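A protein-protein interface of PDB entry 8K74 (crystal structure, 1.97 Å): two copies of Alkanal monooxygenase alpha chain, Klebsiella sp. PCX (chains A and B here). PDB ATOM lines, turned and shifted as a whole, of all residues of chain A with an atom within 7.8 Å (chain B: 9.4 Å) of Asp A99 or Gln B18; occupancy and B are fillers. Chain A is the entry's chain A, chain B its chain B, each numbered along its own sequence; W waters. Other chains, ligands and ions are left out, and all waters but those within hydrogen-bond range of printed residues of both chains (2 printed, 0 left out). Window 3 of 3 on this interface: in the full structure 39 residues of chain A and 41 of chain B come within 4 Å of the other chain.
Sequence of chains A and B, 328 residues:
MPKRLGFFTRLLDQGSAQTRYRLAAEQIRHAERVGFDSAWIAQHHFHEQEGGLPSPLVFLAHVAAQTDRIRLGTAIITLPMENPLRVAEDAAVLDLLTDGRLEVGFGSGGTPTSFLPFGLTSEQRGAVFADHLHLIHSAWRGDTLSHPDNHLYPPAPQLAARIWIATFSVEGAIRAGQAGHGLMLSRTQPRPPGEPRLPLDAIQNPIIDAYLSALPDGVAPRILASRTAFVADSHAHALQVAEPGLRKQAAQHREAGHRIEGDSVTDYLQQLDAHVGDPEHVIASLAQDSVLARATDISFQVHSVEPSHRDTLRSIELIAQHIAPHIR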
ATOM      1  N   ALA A  64      -7.138 -21.752  20.793  1.00  0.00           N
ATOM      2  CA  ALA A  64      -5.882 -21.031  20.943  1.00  0.00           C
ATOM      3  C   ALA A  64      -5.934 -20.071  22.130  1.00  0.00           C
ATOM      4  O   ALA A  64      -4.942 -19.914  22.853  1.00  0.00           O
ATOM      5  CB  ALA A  64      -5.530 -20.280  19.657  1.00  0.00           C
ATOM      6  N   ASP A  68      -1.636 -22.410  25.443  1.00  0.00           N
ATOM      7  CA  ASP A  68      -0.474 -21.533  25.480  1.00  0.00           C
ATOM      8  C   ASP A  68       0.718 -22.092  24.718  1.00  0.00           C
ATOM      9  O   ASP A  68       1.380 -21.375  23.964  1.00  0.00           O
ATOM     10  CB  ASP A  68      -0.079 -21.272  26.932  1.00  0.00           C
ATOM     11  CG  ASP A  68       1.104 -20.369  27.037  1.00  0.00           C
ATOM     12  OD1 ASP A  68       0.970 -19.211  26.598  1.00  0.00           O
ATOM     13  OD2 ASP A  68       2.149 -20.799  27.559  1.00  0.00           O
ATOM     14  N   ARG A  71       1.073 -26.700  19.833  1.00  0.00           N
ATOM     15  CA  ARG A  71       0.839 -26.293  18.458  1.00  0.00           C
ATOM     16  C   ARG A  71      -0.513 -26.804  17.956  1.00  0.00           C
ATOM     17  O   ARG A  71      -1.018 -27.847  18.391  1.00  0.00           O
ATOM     18  CB  ARG A  71       1.975 -26.774  17.561  1.00  0.00           C
ATOM     19  CG  ARG A  71       3.328 -26.215  18.008  1.00  0.00           C
ATOM     20  CD  ARG A  71       4.427 -26.472  16.976  1.00  0.00           C
ATOM     21  NE  ARG A  71       4.251 -25.613  15.813  1.00  0.00           N
ATOM     22  CZ  ARG A  71       4.366 -24.291  15.821  1.00  0.00           C
ATOM     23  NH1 ARG A  71       4.780 -23.637  16.897  1.00  0.00           N
ATOM     24  NH2 ARG A  71       4.054 -23.604  14.721  1.00  0.00           N
ATOM     25  N   ALA A  92      -3.917 -16.714   7.838  1.00  0.00           N
ATOM     26  CA  ALA A  92      -2.991 -15.636   8.175  1.00  0.00           C
ATOM     27  C   ALA A  92      -3.405 -14.919   9.461  1.00  0.00           C
ATOM     28  O   ALA A  92      -2.550 -14.561  10.283  1.00  0.00           O
ATOM     29  CB  ALA A  92      -2.904 -14.641   7.012  1.00  0.00           C
ATOM     30  N   VAL A  93      -4.712 -14.718   9.662  1.00  0.00           N
ATOM     31  CA  VAL A  93      -5.187 -14.100  10.895  1.00  0.00           C
ATOM     32  C   VAL A  93      -4.994 -15.053  12.065  1.00  0.00           C
ATOM     33  O   VAL A  93      -4.504 -14.660  13.132  1.00  0.00           O
ATOM     34  CB  VAL A  93      -6.659 -13.663  10.751  1.00  0.00           C
ATOM     35  CG1 VAL A  93      -7.242 -13.267  12.089  1.00  0.00           C
ATOM     36  CG2 VAL A  93      -6.792 -12.523   9.762  1.00  0.00           C
ATOM     37  N   LEU A  94      -5.371 -16.318  11.877  1.00  0.00           N
ATOM     38  CA  LEU A  94      -5.289 -17.304  12.952  1.00  0.00           C
ATOM     39  C   LEU A  94      -3.862 -17.468  13.461  1.00  0.00           C
ATOM     40  O   LEU A  94      -3.635 -17.549  14.676  1.00  0.00           O
ATOM     41  CB  LEU A  94      -5.824 -18.652  12.468  1.00  0.00           C
ATOM     42  CG  LEU A  94      -5.640 -19.819  13.440  1.00  0.00           C
ATOM     43  CD1 LEU A  94      -6.321 -19.461  14.757  1.00  0.00           C
ATOM     44  CD2 LEU A  94      -6.244 -21.075  12.835  1.00  0.00           C
ATOM     45  N   ASP A  95      -2.889 -17.545  12.559  1.00  0.00           N
ATOM     46  CA  ASP A  95      -1.521 -17.749  13.013  1.00  0.00           C
ATOM     47  C   ASP A  95      -1.096 -16.628  13.953  1.00  0.00           C
ATOM     48  O   ASP A  95      -0.512 -16.886  15.011  1.00  0.00           O
ATOM     49  CB  ASP A  95      -0.575 -17.869  11.830  1.00  0.00           C
ATOM     50  CG  ASP A  95       0.835 -18.252  12.263  1.00  0.00           C
ATOM     51  OD1 ASP A  95       0.961 -19.199  13.059  1.00  0.00           O
ATOM     52  OD2 ASP A  95       1.808 -17.612  11.816  1.00  0.00           O
ATOM     53  N   LEU A  96      -1.466 -15.389  13.629  1.00  0.00           N
ATOM     54  CA  LEU A  96      -1.179 -14.272  14.523  1.00  0.00           C
ATOM     55  C   LEU A  96      -1.905 -14.432  15.854  1.00  0.00           C
ATOM     56  O   LEU A  96      -1.313 -14.224  16.926  1.00  0.00           O
ATOM     57  CB  LEU A  96      -1.565 -12.963  13.839  1.00  0.00           C
ATOM     58  CG  LEU A  96      -0.789 -12.697  12.542  1.00  0.00           C
ATOM     59  CD1 LEU A  96      -1.007 -11.263  12.028  1.00  0.00           C
ATOM     60  CD2 LEU A  96       0.710 -12.948  12.720  1.00  0.00           C
ATOM     61  N   LEU A  97      -3.181 -14.831  15.812  1.00  0.00           N
ATOM     62  CA  LEU A  97      -3.918 -15.058  17.050  1.00  0.00           C
ATOM     63  C   LEU A  97      -3.281 -16.150  17.898  1.00  0.00           C
ATOM     64  O   LEU A  97      -3.322 -16.080  19.131  1.00  0.00           O
ATOM     65  CB  LEU A  97      -5.376 -15.414  16.745  1.00  0.00           C
ATOM     66  CG  LEU A  97      -6.189 -14.332  16.027  1.00  0.00           C
ATOM     67  CD1 LEU A  97      -7.624 -14.792  15.748  1.00  0.00           C
ATOM     68  CD2 LEU A  97      -6.169 -13.019  16.828  1.00  0.00           C
ATOM     69  N   THR A  98      -2.689 -17.163  17.273  1.00  0.00           N
ATOM     70  CA  THR A  98      -2.051 -18.225  18.044  1.00  0.00           C
ATOM     71  C   THR A  98      -0.620 -17.897  18.426  1.00  0.00           C
ATOM     72  O   THR A  98       0.024 -18.728  19.086  1.00  0.00           O
ATOM     73  CB  THR A  98      -2.026 -19.553  17.275  1.00  0.00           C
ATOM     74  OG1 THR A  98      -1.009 -19.494  16.257  1.00  0.00           O
ATOM     75  CG2 THR A  98      -3.383 -19.856  16.660  1.00  0.00           C
ATOM     76  N   ASP A  99      -0.098 -16.732  18.021  1.00  0.00           N
ATOM     77  CA  ASP A  99       1.314 -16.416  18.234  1.00  0.00           C
ATOM     78  C   ASP A  99       2.224 -17.449  17.564  1.00  0.00           C
ATOM     79  O   ASP A  99       3.186 -17.938  18.159  1.00  0.00           O
ATOM     80  CB  ASP A  99       1.621 -16.306  19.730  1.00  0.00           C
ATOM     81  CG  ASP A  99       2.790 -15.395  20.035  1.00  0.00           C
ATOM     82  OD1 ASP A  99       3.151 -14.528  19.200  1.00  0.00           O
ATOM     83  OD2 ASP A  99       3.378 -15.593  21.124  1.00  0.00           O
ATOM     84  N   GLY A 100       1.915 -17.777  16.305  1.00  0.00           N
ATOM     85  CA  GLY A 100       2.797 -18.619  15.523  1.00  0.00           C
ATOM     86  C   GLY A 100       2.759 -20.101  15.834  1.00  0.00           C
ATOM     87  O   GLY A 100       3.754 -20.793  15.604  1.00  0.00           O
ATOM     88  N   ARG A 101       1.633 -20.626  16.325  1.00  0.00           N
ATOM     89  CA  ARG A 101       1.541 -22.043  16.654  1.00  0.00           C
ATOM     90  C   ARG A 101       0.827 -22.865  15.586  1.00  0.00           C
ATOM     91  O   ARG A 101       0.701 -24.088  15.742  1.00  0.00           O
ATOM     92  CB  ARG A 101       0.834 -22.230  17.999  1.00  0.00           C
ATOM     93  CG  ARG A 101       1.638 -21.727  19.215  1.00  0.00           C
ATOM     94  CD  ARG A 101       0.925 -22.000  20.569  1.00  0.00           C
ATOM     95  NE  ARG A 101      -0.248 -21.165  20.813  1.00  0.00           N
ATOM     96  CZ  ARG A 101      -1.397 -21.573  21.333  1.00  0.00           C
ATOM     97  NH1 ARG A 101      -1.602 -22.835  21.675  1.00  0.00           N
ATOM     98  NH2 ARG A 101      -2.364 -20.681  21.545  1.00  0.00           N
ATOM     99  N   LEU A 102       0.383 -22.231  14.509  1.00  0.00           N
ATOM    100  CA  LEU A 102      -0.452 -22.882  13.515  1.00  0.00           C
ATOM    101  C   LEU A 102       0.357 -23.774  12.577  1.00  0.00           C
ATOM    102  O   LEU A 102       1.470 -23.429  12.162  1.00  0.00           O
ATOM    103  CB  LEU A 102      -1.212 -21.818  12.718  1.00  0.00           C
ATOM    104  CG  LEU A 102      -2.167 -22.368  11.649  1.00  0.00           C
ATOM    105  CD1 LEU A 102      -3.250 -23.206  12.275  1.00  0.00           C
ATOM    106  CD2 LEU A 102      -2.776 -21.238  10.819  1.00  0.00           C
ATOM    107  N   TYR A 153      -3.826  -8.892   3.419  1.00  0.00           N
ATOM    108  CA  TYR A 153      -3.651  -8.327   4.760  1.00  0.00           C
ATOM    109  C   TYR A 153      -4.405  -9.209   5.751  1.00  0.00           C
ATOM    110  O   TYR A 153      -5.600  -9.470   5.548  1.00  0.00           O
ATOM    111  CB  TYR A 153      -4.160  -6.864   4.880  1.00  0.00           C
ATOM    112  CG  TYR A 153      -3.758  -6.275   6.221  1.00  0.00           C
ATOM    113  CD1 TYR A 153      -4.551  -6.457   7.362  1.00  0.00           C
ATOM    114  CD2 TYR A 153      -2.538  -5.611   6.369  1.00  0.00           C
ATOM    115  CE1 TYR A 153      -4.148  -5.966   8.598  1.00  0.00           C
ATOM    116  CE2 TYR A 153      -2.134  -5.102   7.615  1.00  0.00           C
ATOM    117  CZ  TYR A 153      -2.949  -5.286   8.720  1.00  0.00           C
ATOM    118  OH  TYR A 153      -2.571  -4.792   9.955  1.00  0.00           O
ATOM    119  N   PRO A 154      -3.767  -9.675   6.843  1.00  0.00           N
ATOM    120  CA  PRO A 154      -2.389  -9.411   7.287  1.00  0.00           C
ATOM    121  C   PRO A 154      -1.419 -10.202   6.446  1.00  0.00           C
ATOM    122  O   PRO A 154      -1.814 -11.230   5.891  1.00  0.00           O
ATOM    123  CB  PRO A 154      -2.400  -9.895   8.743  1.00  0.00           C
ATOM    124  CG  PRO A 154      -3.386 -11.041   8.723  1.00  0.00           C
ATOM    125  CD  PRO A 154      -4.474 -10.559   7.787  1.00  0.00           C
ATOM    126  N   PRO A 155      -0.160  -9.775   6.326  1.00  0.00           N
ATOM    127  CA  PRO A 155       0.817 -10.605   5.620  1.00  0.00           C
ATOM    128  C   PRO A 155       1.019 -11.916   6.355  1.00  0.00           C
ATOM    129  O   PRO A 155       0.817 -12.017   7.567  1.00  0.00           O
ATOM    130  CB  PRO A 155       2.102  -9.753   5.633  1.00  0.00           C
ATOM    131  CG  PRO A 155       1.838  -8.642   6.580  1.00  0.00           C
ATOM    132  CD  PRO A 155       0.370  -8.440   6.639  1.00  0.00           C
ATOM    133  N   GLN A 158       5.357 -16.170   6.722  1.00  0.00           N
ATOM    134  CA  GLN A 158       5.871 -17.313   7.461  1.00  0.00           C
ATOM    135  C   GLN A 158       5.075 -18.594   7.233  1.00  0.00           C
ATOM    136  O   GLN A 158       5.536 -19.670   7.650  1.00  0.00           O
ATOM    137  CB  GLN A 158       5.937 -17.033   8.977  1.00  0.00           C
ATOM    138  CG  GLN A 158       4.622 -16.818   9.821  1.00  0.00           C
ATOM    139  CD  GLN A 158       3.582 -15.820   9.272  1.00  0.00           C
ATOM    140  OE1 GLN A 158       3.905 -14.949   8.460  1.00  0.00           O
ATOM    141  NE2 GLN A 158       2.335 -15.908   9.783  1.00  0.00           N
ATOM    142  N   ARG A 162       4.994 -23.867   6.682  1.00  0.00           N
ATOM    143  CA  ARG A 162       4.261 -24.765   7.573  1.00  0.00           C
ATOM    144  C   ARG A 162       3.074 -25.418   6.872  1.00  0.00           C
ATOM    145  O   ARG A 162       2.050 -25.733   7.504  1.00  0.00           O
ATOM    146  CB  ARG A 162       3.817 -24.028   8.838  1.00  0.00           C
ATOM    147  CG  ARG A 162       4.990 -23.617   9.753  1.00  0.00           C
ATOM    148  CD  ARG A 162       4.410 -22.985  10.989  1.00  0.00           C
ATOM    149  NE  ARG A 162       4.675 -21.554  10.982  1.00  0.00           N
ATOM    150  CZ  ARG A 162       3.928 -20.647  11.593  1.00  0.00           C
ATOM    151  NH1 ARG A 162       2.779 -20.963  12.163  1.00  0.00           N
ATOM    152  NH2 ARG A 162       4.333 -19.382  11.608  1.00  0.00           N
ATOM    153  N   LEU B  11     -10.647  -2.326  13.779  1.00  0.00           N
ATOM    154  CA  LEU B  11      -9.310  -2.819  14.094  1.00  0.00           C
ATOM    155  C   LEU B  11      -8.229  -2.013  13.371  1.00  0.00           C
ATOM    156  O   LEU B  11      -7.417  -2.539  12.607  1.00  0.00           O
ATOM    157  CB  LEU B  11      -9.188  -4.319  13.816  1.00  0.00           C
ATOM    158  CG  LEU B  11     -10.066  -5.197  14.720  1.00  0.00           C
ATOM    159  CD1 LEU B  11     -11.486  -5.372  14.171  1.00  0.00           C
ATOM    160  CD2 LEU B  11      -9.402  -6.543  15.021  1.00  0.00           C
ATOM    161  N   ASP B  13      -6.030   0.255  15.119  1.00  0.00           N
ATOM    162  CA  ASP B  13      -5.015   0.800  16.004  1.00  0.00           C
ATOM    163  C   ASP B  13      -3.638   0.750  15.343  1.00  0.00           C
ATOM    164  O   ASP B  13      -3.372  -0.056  14.443  1.00  0.00           O
ATOM    165  CB  ASP B  13      -5.013   0.039  17.323  1.00  0.00           C
ATOM    166  CG  ASP B  13      -6.308   0.219  18.078  1.00  0.00           C
ATOM    167  OD1 ASP B  13      -7.245  -0.582  17.869  1.00  0.00           O
ATOM    168  OD2 ASP B  13      -6.407   1.206  18.838  1.00  0.00           O
ATOM    169  N   GLN B  14      -2.757   1.648  15.778  1.00  0.00           N
ATOM    170  CA  GLN B  14      -1.422   1.693  15.195  1.00  0.00           C
ATOM    171  C   GLN B  14      -0.631   0.452  15.603  1.00  0.00           C
ATOM    172  O   GLN B  14      -0.611   0.076  16.777  1.00  0.00           O
ATOM    173  CB  GLN B  14      -0.696   2.964  15.638  1.00  0.00           C
ATOM    174  N   GLY B  15       0.007  -0.194  14.628  1.00  0.00           N
ATOM    175  CA  GLY B  15       0.814  -1.375  14.881  1.00  0.00           C
ATOM    176  C   GLY B  15       0.655  -2.455  13.824  1.00  0.00           C
ATOM    177  O   GLY B  15      -0.123  -2.289  12.878  1.00  0.00           O
ATOM    178  N   SER B  16       1.406  -3.553  13.968  1.00  0.00           N
ATOM    179  CA  SER B  16       1.255  -4.727  13.119  1.00  0.00           C
ATOM    180  C   SER B  16      -0.097  -5.386  13.376  1.00  0.00           C
ATOM    181  O   SER B  16      -0.767  -5.131  14.390  1.00  0.00           O
ATOM    182  CB  SER B  16       2.363  -5.737  13.396  1.00  0.00           C
ATOM    183  OG  SER B  16       2.122  -6.364  14.656  1.00  0.00           O
ATOM    184  N   ALA B  17      -0.490  -6.263  12.451  1.00  0.00           N
ATOM    185  CA  ALA B  17      -1.795  -6.893  12.590  1.00  0.00           C
ATOM    186  C   ALA B  17      -1.891  -7.647  13.907  1.00  0.00           C
ATOM    187  O   ALA B  17      -2.932  -7.617  14.568  1.00  0.00           O
ATOM    188  CB  ALA B  17      -2.072  -7.825  11.407  1.00  0.00           C
ATOM    189  N   GLN B  18      -0.813  -8.321  14.319  1.00  0.00           N
ATOM    190  CA  GLN B  18      -0.904  -9.086  15.560  1.00  0.00           C
ATOM    191  C   GLN B  18      -1.173  -8.155  16.731  1.00  0.00           C
ATOM    192  O   GLN B  18      -1.977  -8.468  17.622  1.00  0.00           O
ATOM    193  CB  GLN B  18       0.370  -9.908  15.792  1.00  0.00           C
ATOM    194  CG  GLN B  18       0.253 -10.862  17.000  1.00  0.00           C
ATOM    195  CD  GLN B  18       1.369 -11.890  17.060  1.00  0.00           C
ATOM    196  OE1 GLN B  18       2.187 -11.988  16.144  1.00  0.00           O
ATOM    197  NE2 GLN B  18       1.419 -12.654  18.151  1.00  0.00           N
ATOM    198  N   THR B  19      -0.538  -6.980  16.719  1.00  0.00           N
ATOM    199  CA  THR B  19      -0.795  -5.978  17.750  1.00  0.00           C
ATOM    200  C   THR B  19      -2.223  -5.444  17.667  1.00  0.00           C
ATOM    201  O   THR B  19      -2.891  -5.286  18.698  1.00  0.00           O
ATOM    202  CB  THR B  19       0.222  -4.834  17.619  1.00  0.00           C
ATOM    203  OG1 THR B  19       1.540  -5.357  17.829  1.00  0.00           O
ATOM    204  CG2 THR B  19      -0.042  -3.743  18.645  1.00  0.00           C
ATOM    205  N   ARG B  20      -2.708  -5.147  16.455  1.00  0.00           N
ATOM    206  CA  ARG B  20      -4.096  -4.708  16.308  1.00  0.00           C
ATOM    207  C   ARG B  20      -5.066  -5.721  16.906  1.00  0.00           C
ATOM    208  O   ARG B  20      -6.004  -5.343  17.619  1.00  0.00           O
ATOM    209  CB  ARG B  20      -4.429  -4.457  14.836  1.00  0.00           C
ATOM    210  CG  ARG B  20      -3.792  -3.215  14.246  1.00  0.00           C
ATOM    211  CD  ARG B  20      -3.908  -3.201  12.710  1.00  0.00           C
ATOM    212  NE  ARG B  20      -3.735  -1.855  12.183  1.00  0.00           N
ATOM    213  CZ  ARG B  20      -4.192  -1.428  11.014  1.00  0.00           C
ATOM    214  NH1 ARG B  20      -4.816  -2.237  10.175  1.00  0.00           N
ATOM    215  NH2 ARG B  20      -4.004  -0.158  10.671  1.00  0.00           N
ATOM    216  N   TYR B  21      -4.846  -7.010  16.650  1.00  0.00           N
ATOM    217  CA  TYR B  21      -5.773  -8.030  17.139  1.00  0.00           C
ATOM    218  C   TYR B  21      -5.727  -8.129  18.655  1.00  0.00           C
ATOM    219  O   TYR B  21      -6.758  -8.318  19.318  1.00  0.00           O
ATOM    220  CB  TYR B  21      -5.437  -9.379  16.502  1.00  0.00           C
ATOM    221  CG  TYR B  21      -5.559  -9.370  14.996  1.00  0.00           C
ATOM    222  CD1 TYR B  21      -6.218  -8.335  14.345  1.00  0.00           C
ATOM    223  CD2 TYR B  21      -4.964 -10.371  14.219  1.00  0.00           C
ATOM    224  CE1 TYR B  21      -6.316  -8.309  12.950  1.00  0.00           C
ATOM    225  CE2 TYR B  21      -5.051 -10.350  12.841  1.00  0.00           C
ATOM    226  CZ  TYR B  21      -5.732  -9.320  12.207  1.00  0.00           C
ATOM    227  OH  TYR B  21      -5.818  -9.279  10.821  1.00  0.00           O
ATOM    228  N   ARG B  22      -4.541  -7.980  19.229  1.00  0.00           N
ATOM    229  CA  ARG B  22      -4.454  -8.051  20.680  1.00  0.00           C
ATOM    230  C   ARG B  22      -5.070  -6.812  21.338  1.00  0.00           C
ATOM    231  O   ARG B  22      -5.714  -6.925  22.391  1.00  0.00           O
ATOM    232  CB  ARG B  22      -2.988  -8.290  21.036  1.00  0.00           C
ATOM    233  CG  ARG B  22      -2.558  -8.301  22.469  1.00  0.00           C
ATOM    234  CD  ARG B  22      -1.227  -9.074  22.448  1.00  0.00           C
ATOM    235  NE  ARG B  22      -0.197  -8.299  21.770  1.00  0.00           N
ATOM    236  CZ  ARG B  22       0.745  -8.815  20.989  1.00  0.00           C
ATOM    237  NH1 ARG B  22       0.850 -10.121  20.796  1.00  0.00           N
ATOM    238  NH2 ARG B  22       1.594  -7.997  20.375  1.00  0.00           N
ATOM    239  N   LEU B  23      -4.951  -5.640  20.705  1.00  0.00           N
ATOM    240  CA  LEU B  23      -5.533  -4.430  21.286  1.00  0.00           C
ATOM    241  C   LEU B  23      -7.050  -4.433  21.132  1.00  0.00           C
ATOM    242  O   LEU B  23      -7.783  -4.033  22.050  1.00  0.00           O
ATOM    243  CB  LEU B  23      -4.926  -3.188  20.624  1.00  0.00           C
ATOM    244  CG  LEU B  23      -3.432  -2.888  20.795  1.00  0.00           C
ATOM    245  CD1 LEU B  23      -3.092  -1.605  20.080  1.00  0.00           C
ATOM    246  CD2 LEU B  23      -3.068  -2.758  22.267  1.00  0.00           C
ATOM    247  N   ALA B  24      -7.545  -4.878  19.971  1.00  0.00           N
ATOM    248  CA  ALA B  24      -8.988  -5.031  19.795  1.00  0.00           C
ATOM    249  C   ALA B  24      -9.583  -5.988  20.828  1.00  0.00           C
ATOM    250  O   ALA B  24     -10.632  -5.709  21.419  1.00  0.00           O
ATOM    251  CB  ALA B  24      -9.286  -5.524  18.374  1.00  0.00           C
ATOM    252  N   ALA B  25      -8.934  -7.135  21.048  1.00  0.00           N
ATOM    253  CA  ALA B  25      -9.453  -8.100  22.014  1.00  0.00           C
ATOM    254  C   ALA B  25      -9.522  -7.498  23.413  1.00  0.00           C
ATOM    255  O   ALA B  25     -10.513  -7.676  24.134  1.00  0.00           O
ATOM    256  CB  ALA B  25      -8.573  -9.350  22.027  1.00  0.00           C
ATOM    257  N   GLU B  26      -8.472  -6.783  23.810  1.00  0.00           N
ATOM    258  CA  GLU B  26      -8.475  -6.099  25.100  1.00  0.00           C
ATOM    259  C   GLU B  26      -9.568  -5.033  25.154  1.00  0.00           C
ATOM    260  O   GLU B  26     -10.213  -4.849  26.193  1.00  0.00           O
ATOM    261  CB  GLU B  26      -7.090  -5.493  25.350  1.00  0.00           C
ATOM    262  CG  GLU B  26      -6.902  -4.810  26.707  1.00  0.00           C
ATOM    263  CD  GLU B  26      -5.438  -4.502  27.027  1.00  0.00           C
ATOM    264  OE1 GLU B  26      -4.571  -5.382  26.790  1.00  0.00           O
ATOM    265  OE2 GLU B  26      -5.158  -3.379  27.510  1.00  0.00           O
ATOM    266  N   GLU B  48      -4.730  -2.132   4.873  1.00  0.00           N
ATOM    267  CA  GLU B  48      -4.376  -1.907   6.270  1.00  0.00           C
ATOM    268  C   GLU B  48      -5.048  -0.662   6.841  1.00  0.00           C
ATOM    269  O   GLU B  48      -5.349  -0.615   8.039  1.00  0.00           O
ATOM    270  CB  GLU B  48      -2.846  -1.801   6.355  1.00  0.00           C
ATOM    271  CG  GLU B  48      -2.238  -1.274   7.635  1.00  0.00           C
ATOM    272  CD  GLU B  48      -0.712  -1.341   7.574  1.00  0.00           C
ATOM    273  OE1 GLU B  48      -0.163  -1.243   6.459  1.00  0.00           O
ATOM    274  OE2 GLU B  48      -0.066  -1.556   8.620  1.00  0.00           O
ATOM    275  N   GLY B  52      -8.270  -3.743   9.738  1.00  0.00           N
ATOM    276  CA  GLY B  52      -7.231  -4.728   9.916  1.00  0.00           C
ATOM    277  C   GLY B  52      -7.662  -6.175   9.904  1.00  0.00           C
ATOM    278  O   GLY B  52      -6.819  -7.054  10.122  1.00  0.00           O
ATOM    279  N   PHE B  59     -11.736 -14.215  14.316  1.00  0.00           N
ATOM    280  CA  PHE B  59     -11.365 -13.339  15.428  1.00  0.00           C
ATOM    281  C   PHE B  59     -12.382 -13.422  16.567  1.00  0.00           C
ATOM    282  O   PHE B  59     -12.006 -13.455  17.745  1.00  0.00           O
ATOM    283  CB  PHE B  59     -11.224 -11.900  14.932  1.00  0.00           C
ATOM    284  CG  PHE B  59     -10.958 -10.907  16.037  1.00  0.00           C
ATOM    285  CD1 PHE B  59      -9.670 -10.720  16.511  1.00  0.00           C
ATOM    286  CD2 PHE B  59     -11.989 -10.180  16.607  1.00  0.00           C
ATOM    287  CE1 PHE B  59      -9.415  -9.822  17.550  1.00  0.00           C
ATOM    288  CE2 PHE B  59     -11.739  -9.267  17.628  1.00  0.00           C
ATOM    289  CZ  PHE B  59     -10.454  -9.092  18.096  1.00  0.00           C
ATOM    290  N   HIS B  62     -11.931 -16.315  18.844  1.00  0.00           N
ATOM    291  CA  HIS B  62     -10.866 -16.049  19.806  1.00  0.00           C
ATOM    292  C   HIS B  62     -11.370 -15.188  20.965  1.00  0.00           C
ATOM    293  O   HIS B  62     -11.171 -15.520  22.146  1.00  0.00           O
ATOM    294  CB  HIS B  62      -9.716 -15.354  19.076  1.00  0.00           C
ATOM    295  CG  HIS B  62      -8.439 -15.292  19.855  1.00  0.00           C
ATOM    296  ND1 HIS B  62      -7.605 -16.382  20.011  1.00  0.00           N
ATOM    297  CD2 HIS B  62      -7.860 -14.274  20.532  1.00  0.00           C
ATOM    298  CE1 HIS B  62      -6.556 -16.029  20.734  1.00  0.00           C
ATOM    299  NE2 HIS B  62      -6.687 -14.755  21.063  1.00  0.00           N
HETATM  300  O   HOH W   1       2.998 -14.811  15.803  1.00  0.00           O
HETATM  301  O   HOH W   2      -0.642  -3.243  10.461  1.00  0.00           O
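The backbone carbonyl oxygen (O) of Leu A96 is in hydrogen-bond range of the side-chain amide nitrogen (NE2) of Gln B18 (3.4 Å). OD1 of Asp A99 is in hydrogen-bond range of NE2 of Gln B18 (2.8 Å). NH1 of Arg B20 lies within hydrogen-bond range of OH of Tyr A153 (3.4 Å).
The backbone carbonyl oxygen (O) of Glu B48 sits at hydrogen-bond distance from the guanidinium group (NH1) of Arg B20 (2.7 Å). The side-chain hydroxyl (OH) of Tyr B21 is in hydrogen-bond range of the backbone carbonyl oxygen (O) of Gly B52, at 2.5 Å. The backbone carbonyl oxygen (O) of Leu B11 lies within hydrogen-bond range of the backbone NH (N) of Gly B52 (3.2 Å). NE of Arg B20 is in hydrogen-bond range of O of Asp B13 (2.9 Å).
Among the printed residues, merely in contact across the chains: Val A93 with Tyr B21 (3.5 Å), Leu A96 with Ala B17 (3.7 Å), Leu A97 with Tyr B21 (3.7 Å), Leu A97 with His B62 (3.6 Å), Tyr A153 with Ala B17 (3.4 Å), Tyr A153 with Glu B48 (3.6 Å), Tyr A153 with Gly B52 (3.3 Å), Pro A154 with Ala B17 (3.4 Å) and Pro A154 with Tyr B21 (3.6 Å).
Asp A99 touches just one residue of chain B: Gln B18 (2.8 Å). Of the printed residues of chain A, Gln B18 touches Leu A96 (3.4 Å) and Asp A99 (2.8 Å). Leu A96 touches just these residues of chain B: Ala B17 (3.7 Å) and Gln B18 (3.4 Å). No residue of chain B comes within 4 Å of Thr A98. Of chain A, only Leu A96, Tyr A153 and Pro A154 come within 4 Å of Ala B17. Of the printed residues of chain A, Gly B52 touches Tyr A153 (3.3 Å). Of the printed residues of chain A, His B62 touches Leu A97 (3.6 Å). The nearest residue of chain B that does not touch Asp A99 is Arg B22 (5.2 Å). The nearest printed residue of chain A that does not touch Tyr B21 is Leu A96 (4.2 Å).
Of the 19 printed residues of chain B, 7 touch a printed residue of chain A. Hydrophobic or aromatic side chains of chain B that line the printed part of chain A: Ala B17, Tyr B21 and His B62. Among the printed residues, no Asp or Glu carboxylate lies within 4 Å of a Lys or Arg side-chain nitrogen of the other chain.
No position is printed for both chains. Of the 12 pairs that touch across the chains among the printed residues, none has its exchanged pair printed and touching as well.
Water W2 lies within hydrogen-bond range of the side-chain hydroxyl of Tyr A153 (2.5 Å), the side-chain carboxylate of Glu B48 (2.6 Å) and the backbone carbonyl oxygen of Gly B15 (2.6 Å). Water W1 lies within hydrogen-bond range of OE1 of Gln B18 (3.0 Å), N of Gly A100 (3.2 Å) and OD1 of Asp A99 (3.4 Å).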
